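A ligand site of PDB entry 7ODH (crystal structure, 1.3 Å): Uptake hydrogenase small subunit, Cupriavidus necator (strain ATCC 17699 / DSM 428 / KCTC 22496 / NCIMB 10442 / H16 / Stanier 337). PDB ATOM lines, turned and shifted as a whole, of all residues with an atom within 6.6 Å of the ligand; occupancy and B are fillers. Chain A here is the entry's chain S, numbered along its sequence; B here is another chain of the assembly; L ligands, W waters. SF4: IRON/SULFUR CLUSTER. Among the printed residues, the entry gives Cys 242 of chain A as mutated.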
ATOM      1  N   GLY A 148      12.489 -26.879   7.363  1.00  0.00           N
ATOM      2  CA  GLY A 148      11.122 -26.567   7.772  1.00  0.00           C
ATOM      3  C   GLY A 148      10.250 -26.438   6.556  1.00  0.00           C
ATOM      4  O   GLY A 148      10.752 -26.090   5.468  1.00  0.00           O
ATOM      5  N   CYS A 149       8.956 -26.698   6.714  1.00  0.00           N
ATOM      6  CA  CYS A 149       8.006 -26.763   5.595  1.00  0.00           C
ATOM      7  C   CYS A 149       6.820 -25.858   5.884  1.00  0.00           C
ATOM      8  O   CYS A 149       5.739 -26.326   6.258  1.00  0.00           O
ATOM      9  CB  CYS A 149       7.575 -28.204   5.360  1.00  0.00           C
ATOM     10  SG  CYS A 149       6.696 -28.378   3.796  1.00  0.00           S
ATOM     11  N   PRO A 150       6.957 -24.517   5.766  1.00  0.00           N
ATOM     12  CA  PRO A 150       8.217 -23.832   5.525  1.00  0.00           C
ATOM     13  C   PRO A 150       8.943 -23.542   6.832  1.00  0.00           C
ATOM     14  O   PRO A 150       8.410 -23.796   7.904  1.00  0.00           O
ATOM     15  CB  PRO A 150       7.764 -22.508   4.906  1.00  0.00           C
ATOM     16  CG  PRO A 150       6.433 -22.215   5.591  1.00  0.00           C
ATOM     17  CD  PRO A 150       5.830 -23.573   5.898  1.00  0.00           C
ATOM     18  N   ILE A 152      10.072 -20.875   9.764  1.00  0.00           N
ATOM     19  CA  ILE A 152       9.459 -19.680  10.398  1.00  0.00           C
ATOM     20  C   ILE A 152       9.940 -18.429   9.649  1.00  0.00           C
ATOM     21  O   ILE A 152      11.120 -18.360   9.285  1.00  0.00           O
ATOM     22  CB  ILE A 152       9.811 -19.622  11.893  1.00  0.00           C
ATOM     23  CG1 ILE A 152       9.303 -20.863  12.635  1.00  0.00           C
ATOM     24  CG2 ILE A 152       9.299 -18.337  12.526  1.00  0.00           C
ATOM     25  CD1 ILE A 152       9.902 -21.029  14.008  1.00  0.00           C
ATOM     26  N   ILE A 186      11.736 -28.893  19.775  1.00  0.00           N
ATOM     27  CA  ILE A 186      10.383 -28.348  20.090  1.00  0.00           C
ATOM     28  C   ILE A 186      10.045 -28.706  21.548  1.00  0.00           C
ATOM     29  O   ILE A 186       9.556 -27.827  22.281  1.00  0.00           O
ATOM     30  CB  ILE A 186       9.337 -28.908  19.109  1.00  0.00           C
ATOM     31  CG1 ILE A 186       9.664 -28.576  17.651  1.00  0.00           C
ATOM     32  CG2 ILE A 186       7.941 -28.459  19.488  1.00  0.00           C
ATOM     33  CD1 ILE A 186       9.744 -27.092  17.374  1.00  0.00           C
ATOM     34  N   LYS A 222       5.803 -35.158  17.216  1.00  0.00           N
ATOM     35  CA  LYS A 222       7.224 -35.484  16.951  1.00  0.00           C
ATOM     36  C   LYS A 222       8.117 -34.362  17.515  1.00  0.00           C
ATOM     37  O   LYS A 222       9.304 -34.346  17.199  1.00  0.00           O
ATOM     38  CB  LYS A 222       7.427 -35.727  15.460  1.00  0.00           C
ATOM     39  CG  LYS A 222       6.607 -36.884  14.894  1.00  0.00           C
ATOM     40  CD  LYS A 222       6.677 -38.131  15.758  1.00  0.00           C
ATOM     41  CE  LYS A 222       6.114 -39.387  15.119  1.00  0.00           C
ATOM     42  NZ  LYS A 222       4.699 -39.216  14.685  1.00  0.00           N
ATOM     43  N   GLY A 223       7.569 -33.515  18.383  1.00  0.00           N
ATOM     44  CA  GLY A 223       8.344 -32.465  19.075  1.00  0.00           C
ATOM     45  C   GLY A 223       9.610 -33.003  19.745  1.00  0.00           C
ATOM     46  O   GLY A 223      10.643 -32.346  19.710  1.00  0.00           O
ATOM     47  N   THR A 226      12.462 -33.209  17.020  1.00  0.00           N
ATOM     48  CA  THR A 226      12.432 -32.156  15.979  1.00  0.00           C
ATOM     49  C   THR A 226      13.116 -30.883  16.486  1.00  0.00           C
ATOM     50  O   THR A 226      12.683 -30.352  17.523  1.00  0.00           O
ATOM     51  CB  THR A 226      10.987 -31.899  15.540  1.00  0.00           C
ATOM     52  OG1 THR A 226      10.441 -33.124  15.075  1.00  0.00           O
ATOM     53  CG2 THR A 226      10.887 -30.852  14.456  1.00  0.00           C
ATOM     54  N   TYR A 227      14.118 -30.405  15.768  1.00  0.00           N
ATOM     55  CA  TYR A 227      14.849 -29.149  16.080  1.00  0.00           C
ATOM     56  C   TYR A 227      14.251 -28.005  15.269  1.00  0.00           C
ATOM     57  O   TYR A 227      14.292 -28.027  14.030  1.00  0.00           O
ATOM     58  CB  TYR A 227      16.337 -29.305  15.790  1.00  0.00           C
ATOM     59  CG  TYR A 227      17.063 -30.204  16.764  1.00  0.00           C
ATOM     60  CD1 TYR A 227      17.026 -31.584  16.619  1.00  0.00           C
ATOM     61  CD2 TYR A 227      17.769 -29.681  17.827  1.00  0.00           C
ATOM     62  CE1 TYR A 227      17.698 -32.414  17.503  1.00  0.00           C
ATOM     63  CE2 TYR A 227      18.440 -30.487  18.719  1.00  0.00           C
ATOM     64  CZ  TYR A 227      18.401 -31.860  18.562  1.00  0.00           C
ATOM     65  OH  TYR A 227      19.060 -32.662  19.441  1.00  0.00           O
ATOM     66  N   ASN A 228      13.729 -27.000  15.972  1.00  0.00           N
ATOM     67  CA  ASN A 228      13.187 -25.772  15.356  1.00  0.00           C
ATOM     68  C   ASN A 228      12.940 -24.764  16.470  1.00  0.00           C
ATOM     69  O   ASN A 228      13.063 -25.137  17.650  1.00  0.00           O
ATOM     70  CB  ASN A 228      11.927 -26.072  14.541  1.00  0.00           C
ATOM     71  CG  ASN A 228      11.741 -25.140  13.350  1.00  0.00           C
ATOM     72  OD1 ASN A 228      12.214 -24.002  13.360  1.00  0.00           O
ATOM     73  ND2 ASN A 228      11.029 -25.621  12.343  1.00  0.00           N
ATOM     74  N   ALA A 229      12.542 -23.542  16.118  1.00  0.00           N
ATOM     75  CA  ALA A 229      12.307 -22.446  17.092  1.00  0.00           C
ATOM     76  C   ALA A 229      10.810 -22.272  17.378  1.00  0.00           C
ATOM     77  O   ALA A 229      10.441 -21.289  18.021  1.00  0.00           O
ATOM     78  CB  ALA A 229      12.928 -21.179  16.563  1.00  0.00           C
ATOM     79  N   CYS A 230       9.965 -23.211  16.958  1.00  0.00           N
ATOM     80  CA  CYS A 230       8.491 -23.047  16.964  1.00  0.00           C
ATOM     81  C   CYS A 230       7.938 -22.844  18.371  1.00  0.00           C
ATOM     82  O   CYS A 230       6.943 -22.130  18.502  1.00  0.00           O
ATOM     83  CB  CYS A 230       7.805 -24.227  16.313  1.00  0.00           C
ATOM     84  SG  CYS A 230       8.458 -24.544  14.660  1.00  0.00           S
ATOM     85  N   SER A 231       8.522 -23.462  19.400  1.00  0.00           N
ATOM     86  CA  SER A 231       7.976 -23.451  20.779  1.00  0.00           C
ATOM     87  C   SER A 231       8.177 -22.075  21.437  1.00  0.00           C
ATOM     88  O   SER A 231       7.443 -21.776  22.380  1.00  0.00           O
ATOM     89  CB  SER A 231       8.590 -24.524  21.627  1.00  0.00           C
ATOM     90  OG  SER A 231       8.164 -25.800  21.201  1.00  0.00           O
ATOM     91  N   TRP A 235       4.988 -18.705  15.432  1.00  0.00           N
ATOM     92  CA  TRP A 235       4.632 -18.450  14.015  1.00  0.00           C
ATOM     93  C   TRP A 235       3.829 -17.168  13.876  1.00  0.00           C
ATOM     94  O   TRP A 235       2.963 -16.891  14.723  1.00  0.00           O
ATOM     95  CB  TRP A 235       3.843 -19.634  13.468  1.00  0.00           C
ATOM     96  CG  TRP A 235       4.737 -20.751  13.043  1.00  0.00           C
ATOM     97  CD1 TRP A 235       5.304 -21.711  13.840  1.00  0.00           C
ATOM     98  CD2 TRP A 235       5.205 -20.988  11.715  1.00  0.00           C
ATOM     99  NE1 TRP A 235       6.097 -22.538  13.078  1.00  0.00           N
ATOM    100  CE2 TRP A 235       6.054 -22.109  11.774  1.00  0.00           C
ATOM    101  CE3 TRP A 235       4.997 -20.351  10.490  1.00  0.00           C
ATOM    102  CZ2 TRP A 235       6.684 -22.625  10.640  1.00  0.00           C
ATOM    103  CZ3 TRP A 235       5.619 -20.856   9.374  1.00  0.00           C
ATOM    104  CH2 TRP A 235       6.460 -21.966   9.451  1.00  0.00           C
ATOM    105  N   PHE A 241       1.720 -21.867  17.364  1.00  0.00           N
ATOM    106  CA  PHE A 241       2.456 -22.914  16.636  1.00  0.00           C
ATOM    107  C   PHE A 241       1.574 -24.156  16.630  1.00  0.00           C
ATOM    108  O   PHE A 241       0.493 -24.155  17.241  1.00  0.00           O
ATOM    109  CB  PHE A 241       3.872 -23.119  17.177  1.00  0.00           C
ATOM    110  CG  PHE A 241       4.012 -23.810  18.517  1.00  0.00           C
ATOM    111  CD1 PHE A 241       3.534 -23.221  19.672  1.00  0.00           C
ATOM    112  CD2 PHE A 241       4.735 -24.988  18.630  1.00  0.00           C
ATOM    113  CE1 PHE A 241       3.722 -23.820  20.910  1.00  0.00           C
ATOM    114  CE2 PHE A 241       4.933 -25.583  19.868  1.00  0.00           C
ATOM    115  CZ  PHE A 241       4.419 -25.004  20.997  1.00  0.00           C
ATOM    116  N   CYS A 242       2.005 -25.180  15.922  1.00  0.00           N
ATOM    117  CA  CYS A 242       1.176 -26.390  15.677  1.00  0.00           C
ATOM    118  C   CYS A 242       0.544 -26.862  16.999  1.00  0.00           C
ATOM    119  O   CYS A 242      -0.681 -27.031  17.068  1.00  0.00           O
ATOM    120  CB  CYS A 242       2.042 -27.459  15.048  1.00  0.00           C
ATOM    121  SG  CYS A 242       2.742 -26.892  13.483  1.00  0.00           S
ATOM    122  N   ILE A 243       1.370 -27.027  18.026  1.00  0.00           N
ATOM    123  CA  ILE A 243       0.934 -27.641  19.309  1.00  0.00           C
ATOM    124  C   ILE A 243      -0.015 -26.688  20.047  1.00  0.00           C
ATOM    125  O   ILE A 243      -1.027 -27.161  20.579  1.00  0.00           O
ATOM    126  CB  ILE A 243       2.182 -28.016  20.112  1.00  0.00           C
ATOM    127  CG1 ILE A 243       2.876 -29.240  19.486  1.00  0.00           C
ATOM    128  CG2 ILE A 243       1.850 -28.248  21.578  1.00  0.00           C
ATOM    129  CD1 ILE A 243       4.372 -29.233  19.620  1.00  0.00           C
ATOM    130  N   HIS A 247      -2.556 -29.414  17.270  1.00  0.00           N
ATOM    131  CA  HIS A 247      -2.036 -30.542  16.447  1.00  0.00           C
ATOM    132  C   HIS A 247      -0.608 -30.855  16.869  1.00  0.00           C
ATOM    133  O   HIS A 247       0.166 -29.919  17.091  1.00  0.00           O
ATOM    134  CB  HIS A 247      -2.128 -30.230  14.942  1.00  0.00           C
ATOM    135  CG  HIS A 247      -2.046 -31.432  14.063  1.00  0.00           C
ATOM    136  ND1 HIS A 247      -0.873 -32.147  13.864  1.00  0.00           N
ATOM    137  CD2 HIS A 247      -2.990 -32.044  13.322  1.00  0.00           C
ATOM    138  CE1 HIS A 247      -1.117 -33.150  13.044  1.00  0.00           C
ATOM    139  NE2 HIS A 247      -2.403 -33.115  12.700  1.00  0.00           N
ATOM    140  N   GLY A 248      -0.251 -32.131  16.983  1.00  0.00           N
ATOM    141  CA  GLY A 248       1.144 -32.488  17.249  1.00  0.00           C
ATOM    142  C   GLY A 248       2.074 -31.944  16.182  1.00  0.00           C
ATOM    143  O   GLY A 248       1.657 -31.778  15.019  1.00  0.00           O
ATOM    144  N   CYS A 249       3.312 -31.674  16.545  1.00  0.00           N
ATOM    145  CA  CYS A 249       4.410 -31.468  15.588  1.00  0.00           C
ATOM    146  C   CYS A 249       4.473 -32.687  14.666  1.00  0.00           C
ATOM    147  O   CYS A 249       4.405 -33.821  15.174  1.00  0.00           O
ATOM    148  CB  CYS A 249       5.712 -31.244  16.368  1.00  0.00           C
ATOM    149  SG  CYS A 249       7.194 -31.100  15.347  1.00  0.00           S
ATOM    150  N   ILE A 250       4.572 -32.477  13.341  1.00  0.00           N
ATOM    151  CA  ILE A 250       4.717 -33.592  12.363  1.00  0.00           C
ATOM    152  C   ILE A 250       6.199 -33.757  11.990  1.00  0.00           C
ATOM    153  O   ILE A 250       6.504 -34.654  11.193  1.00  0.00           O
ATOM    154  CB  ILE A 250       3.819 -33.379  11.122  1.00  0.00           C
ATOM    155  CG1 ILE A 250       4.282 -32.232  10.228  1.00  0.00           C
ATOM    156  CG2 ILE A 250       2.367 -33.223  11.553  1.00  0.00           C
ATOM    157  CD1 ILE A 250       3.540 -32.155   8.899  1.00  0.00           C
ATOM    158  N   GLY A 251       7.088 -32.963  12.588  1.00  0.00           N
ATOM    159  CA  GLY A 251       8.549 -33.127  12.437  1.00  0.00           C
ATOM    160  C   GLY A 251       9.095 -32.431  11.208  1.00  0.00           C
ATOM    161  O   GLY A 251      10.133 -32.881  10.678  1.00  0.00           O
ATOM    162  N   CYS A 252       8.457 -31.334  10.762  1.00  0.00           N
ATOM    163  CA  CYS A 252       8.603 -30.850   9.366  1.00  0.00           C
ATOM    164  C   CYS A 252       9.988 -30.227   9.084  1.00  0.00           C
ATOM    165  O   CYS A 252      10.300 -30.016   7.903  1.00  0.00           O
ATOM    166  CB  CYS A 252       7.477 -29.910   8.955  1.00  0.00           C
ATOM    167  SG  CYS A 252       7.603 -28.192   9.542  1.00  0.00           S
ATOM    168  N   SER A 253      10.813 -29.962  10.095  1.00  0.00           N
ATOM    169  CA  SER A 253      12.179 -29.436   9.872  1.00  0.00           C
ATOM    170  C   SER A 253      13.214 -30.562   9.824  1.00  0.00           C
ATOM    171  O   SER A 253      14.392 -30.246   9.587  1.00  0.00           O
ATOM    172  CB  SER A 253      12.530 -28.420  10.916  1.00  0.00           C
ATOM    173  OG  SER A 253      12.373 -28.964  12.204  1.00  0.00           O
ATOM    174  N   GLU A 254      12.811 -31.817  10.025  1.00  0.00           N
ATOM    175  CA  GLU A 254      13.769 -32.956  10.086  1.00  0.00           C
ATOM    176  C   GLU A 254      13.831 -33.691   8.733  1.00  0.00           C
ATOM    177  O   GLU A 254      12.789 -33.893   8.093  1.00  0.00           O
ATOM    178  CB  GLU A 254      13.410 -33.921  11.217  1.00  0.00           C
ATOM    179  CG  GLU A 254      13.615 -33.306  12.593  1.00  0.00           C
ATOM    180  CD  GLU A 254      15.053 -32.931  12.922  1.00  0.00           C
ATOM    181  OE1 GLU A 254      15.961 -33.704  12.576  1.00  0.00           O
ATOM    182  OE2 GLU A 254      15.249 -31.857  13.530  1.00  0.00           O
ATOM    183  N   ARG B  73       1.035 -29.739   0.639  1.00  0.00           N
ATOM    184  CA  ARG B  73       2.338 -29.323   0.057  1.00  0.00           C
ATOM    185  C   ARG B  73       2.311 -29.421  -1.474  1.00  0.00           C
ATOM    186  O   ARG B  73       3.348 -29.164  -2.090  1.00  0.00           O
ATOM    187  CB  ARG B  73       3.488 -30.136   0.663  1.00  0.00           C
ATOM    188  CG  ARG B  73       4.012 -29.560   1.962  1.00  0.00           C
ATOM    189  CD  ARG B  73       3.007 -29.591   3.093  1.00  0.00           C
ATOM    190  NE  ARG B  73       3.649 -29.144   4.315  1.00  0.00           N
ATOM    191  CZ  ARG B  73       3.111 -29.173   5.525  1.00  0.00           C
ATOM    192  NH1 ARG B  73       1.924 -29.720   5.734  1.00  0.00           N
ATOM    193  NH2 ARG B  73       3.778 -28.622   6.537  1.00  0.00           N
ATOM    194  N   LYS B 226      -0.141 -22.275  12.165  1.00  0.00           N
ATOM    195  CA  LYS B 226       0.903 -21.621  11.343  1.00  0.00           C
ATOM    196  C   LYS B 226       0.360 -21.265   9.961  1.00  0.00           C
ATOM    197  O   LYS B 226      -0.598 -21.907   9.497  1.00  0.00           O
ATOM    198  CB  LYS B 226       2.139 -22.509  11.196  1.00  0.00           C
ATOM    199  CG  LYS B 226       1.867 -23.920  10.691  1.00  0.00           C
ATOM    200  CD  LYS B 226       3.106 -24.795  10.717  1.00  0.00           C
ATOM    201  CE  LYS B 226       3.965 -24.638   9.483  1.00  0.00           C
ATOM    202  NZ  LYS B 226       3.499 -25.515   8.391  1.00  0.00           N
ATOM    203  N   ASN B 231      -2.574 -26.629   9.921  1.00  0.00           N
ATOM    204  CA  ASN B 231      -2.954 -28.035  10.153  1.00  0.00           C
ATOM    205  C   ASN B 231      -4.462 -28.233  10.037  1.00  0.00           C
ATOM    206  O   ASN B 231      -5.233 -27.373  10.462  1.00  0.00           O
ATOM    207  CB  ASN B 231      -2.438 -28.510  11.502  1.00  0.00           C
ATOM    208  CG  ASN B 231      -0.928 -28.397  11.576  1.00  0.00           C
ATOM    209  OD1 ASN B 231      -0.229 -28.930  10.713  1.00  0.00           O
ATOM    210  ND2 ASN B 231      -0.434 -27.662  12.555  1.00  0.00           N
HETATM  211 FE1  SF4 L   1       7.124 -28.026  11.736  1.00  0.00          FE
HETATM  212 FE2  SF4 L   1       4.971 -27.416  13.376  1.00  0.00          FE
HETATM  213 FE3  SF4 L   1       7.429 -26.473  13.983  1.00  0.00          FE
HETATM  214 FE4  SF4 L   1       6.920 -29.113  14.231  1.00  0.00          FE
HETATM  215  S1  SF4 L   1       5.973 -27.435  15.434  1.00  0.00           S
HETATM  216  S2  SF4 L   1       8.779 -28.221  13.326  1.00  0.00           S
HETATM  217  S3  SF4 L   1       5.509 -29.438  12.437  1.00  0.00           S
HETATM  218  S4  SF4 L   1       6.188 -25.981  12.104  1.00  0.00           S
HETATM  219  O   HOH W   1       2.421 -29.466  11.230  1.00  0.00           O
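SG of Cys 249 is bound to FE4 of the ligand (2.3 Å). The side-chain sulfur of Cys 230 is bound to an iron atom (FE3) of the ligand (2.3 Å). The backbone NH of Ile 250 lies close to a sulfur (S3) of the ligand (3.3 Å). The side-chain sulfur of Cys 252 binds an iron atom (FE1) of the ligand (2.3 Å). A sulfur (S2) of the ligand sits close to the side-chain amide nitrogen of Asn 228, 3.6 Å away. The side-chain sulfur of Cys 242 is bound to an iron atom (FE2) of the ligand (2.3 Å). The indole nitrogen (NE1) of Trp 235 sits close to a sulfur (S4) of the ligand (3.6 Å).
Water W1 bridges OD1 of Asn 231 of chain B (2.8 Å) and S3 of the ligand (3.3 Å).
Merely in contact with the ligand: Thr 226 of chain A, Lys 226 of chain B, Ser 253 and Gly 251. Hydrophobic or aromatic side chains that line the ligand: Trp 235 and Ile 250. Within 4 Å of the ligand: Thr 226 of chain A, Asn 228, Cys 230, Trp 235, Cys 242, Cys 249, Ile 250, Gly 251, Cys 252, Ser 253 and Lys 226 of chain B.
ND2 of Asn 231 of chain B lies close to SG of Cys 242, 3.4 Å away. The backbone carbonyl oxygen (O) of Cys 242 sits at hydrogen-bond distance from the backbone NH (N) of His 247 (3.0 Å). NZ of Lys 226 of chain B is in hydrogen-bond range of O of Cys 149. SG of Cys 230 sits close to ND2 of Asn 228 (3.6 Å). The indole nitrogen (NE1) of Trp 235 sits close to the side-chain sulfur (SG) of Cys 230. The side-chain hydroxyl (OG1) of Thr 226 of chain A lies within hydrogen-bond range of the backbone carbonyl oxygen (O) of Lys 222. The backbone carbonyl oxygen (O) of Thr 226 of chain A sits at hydrogen-bond distance from the backbone NH (N) of Ile 186 (2.8 Å). The backbone carbonyl oxygen of Cys 249 is in hydrogen-bond range of the backbone NH of Lys 222 (2.8 Å).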
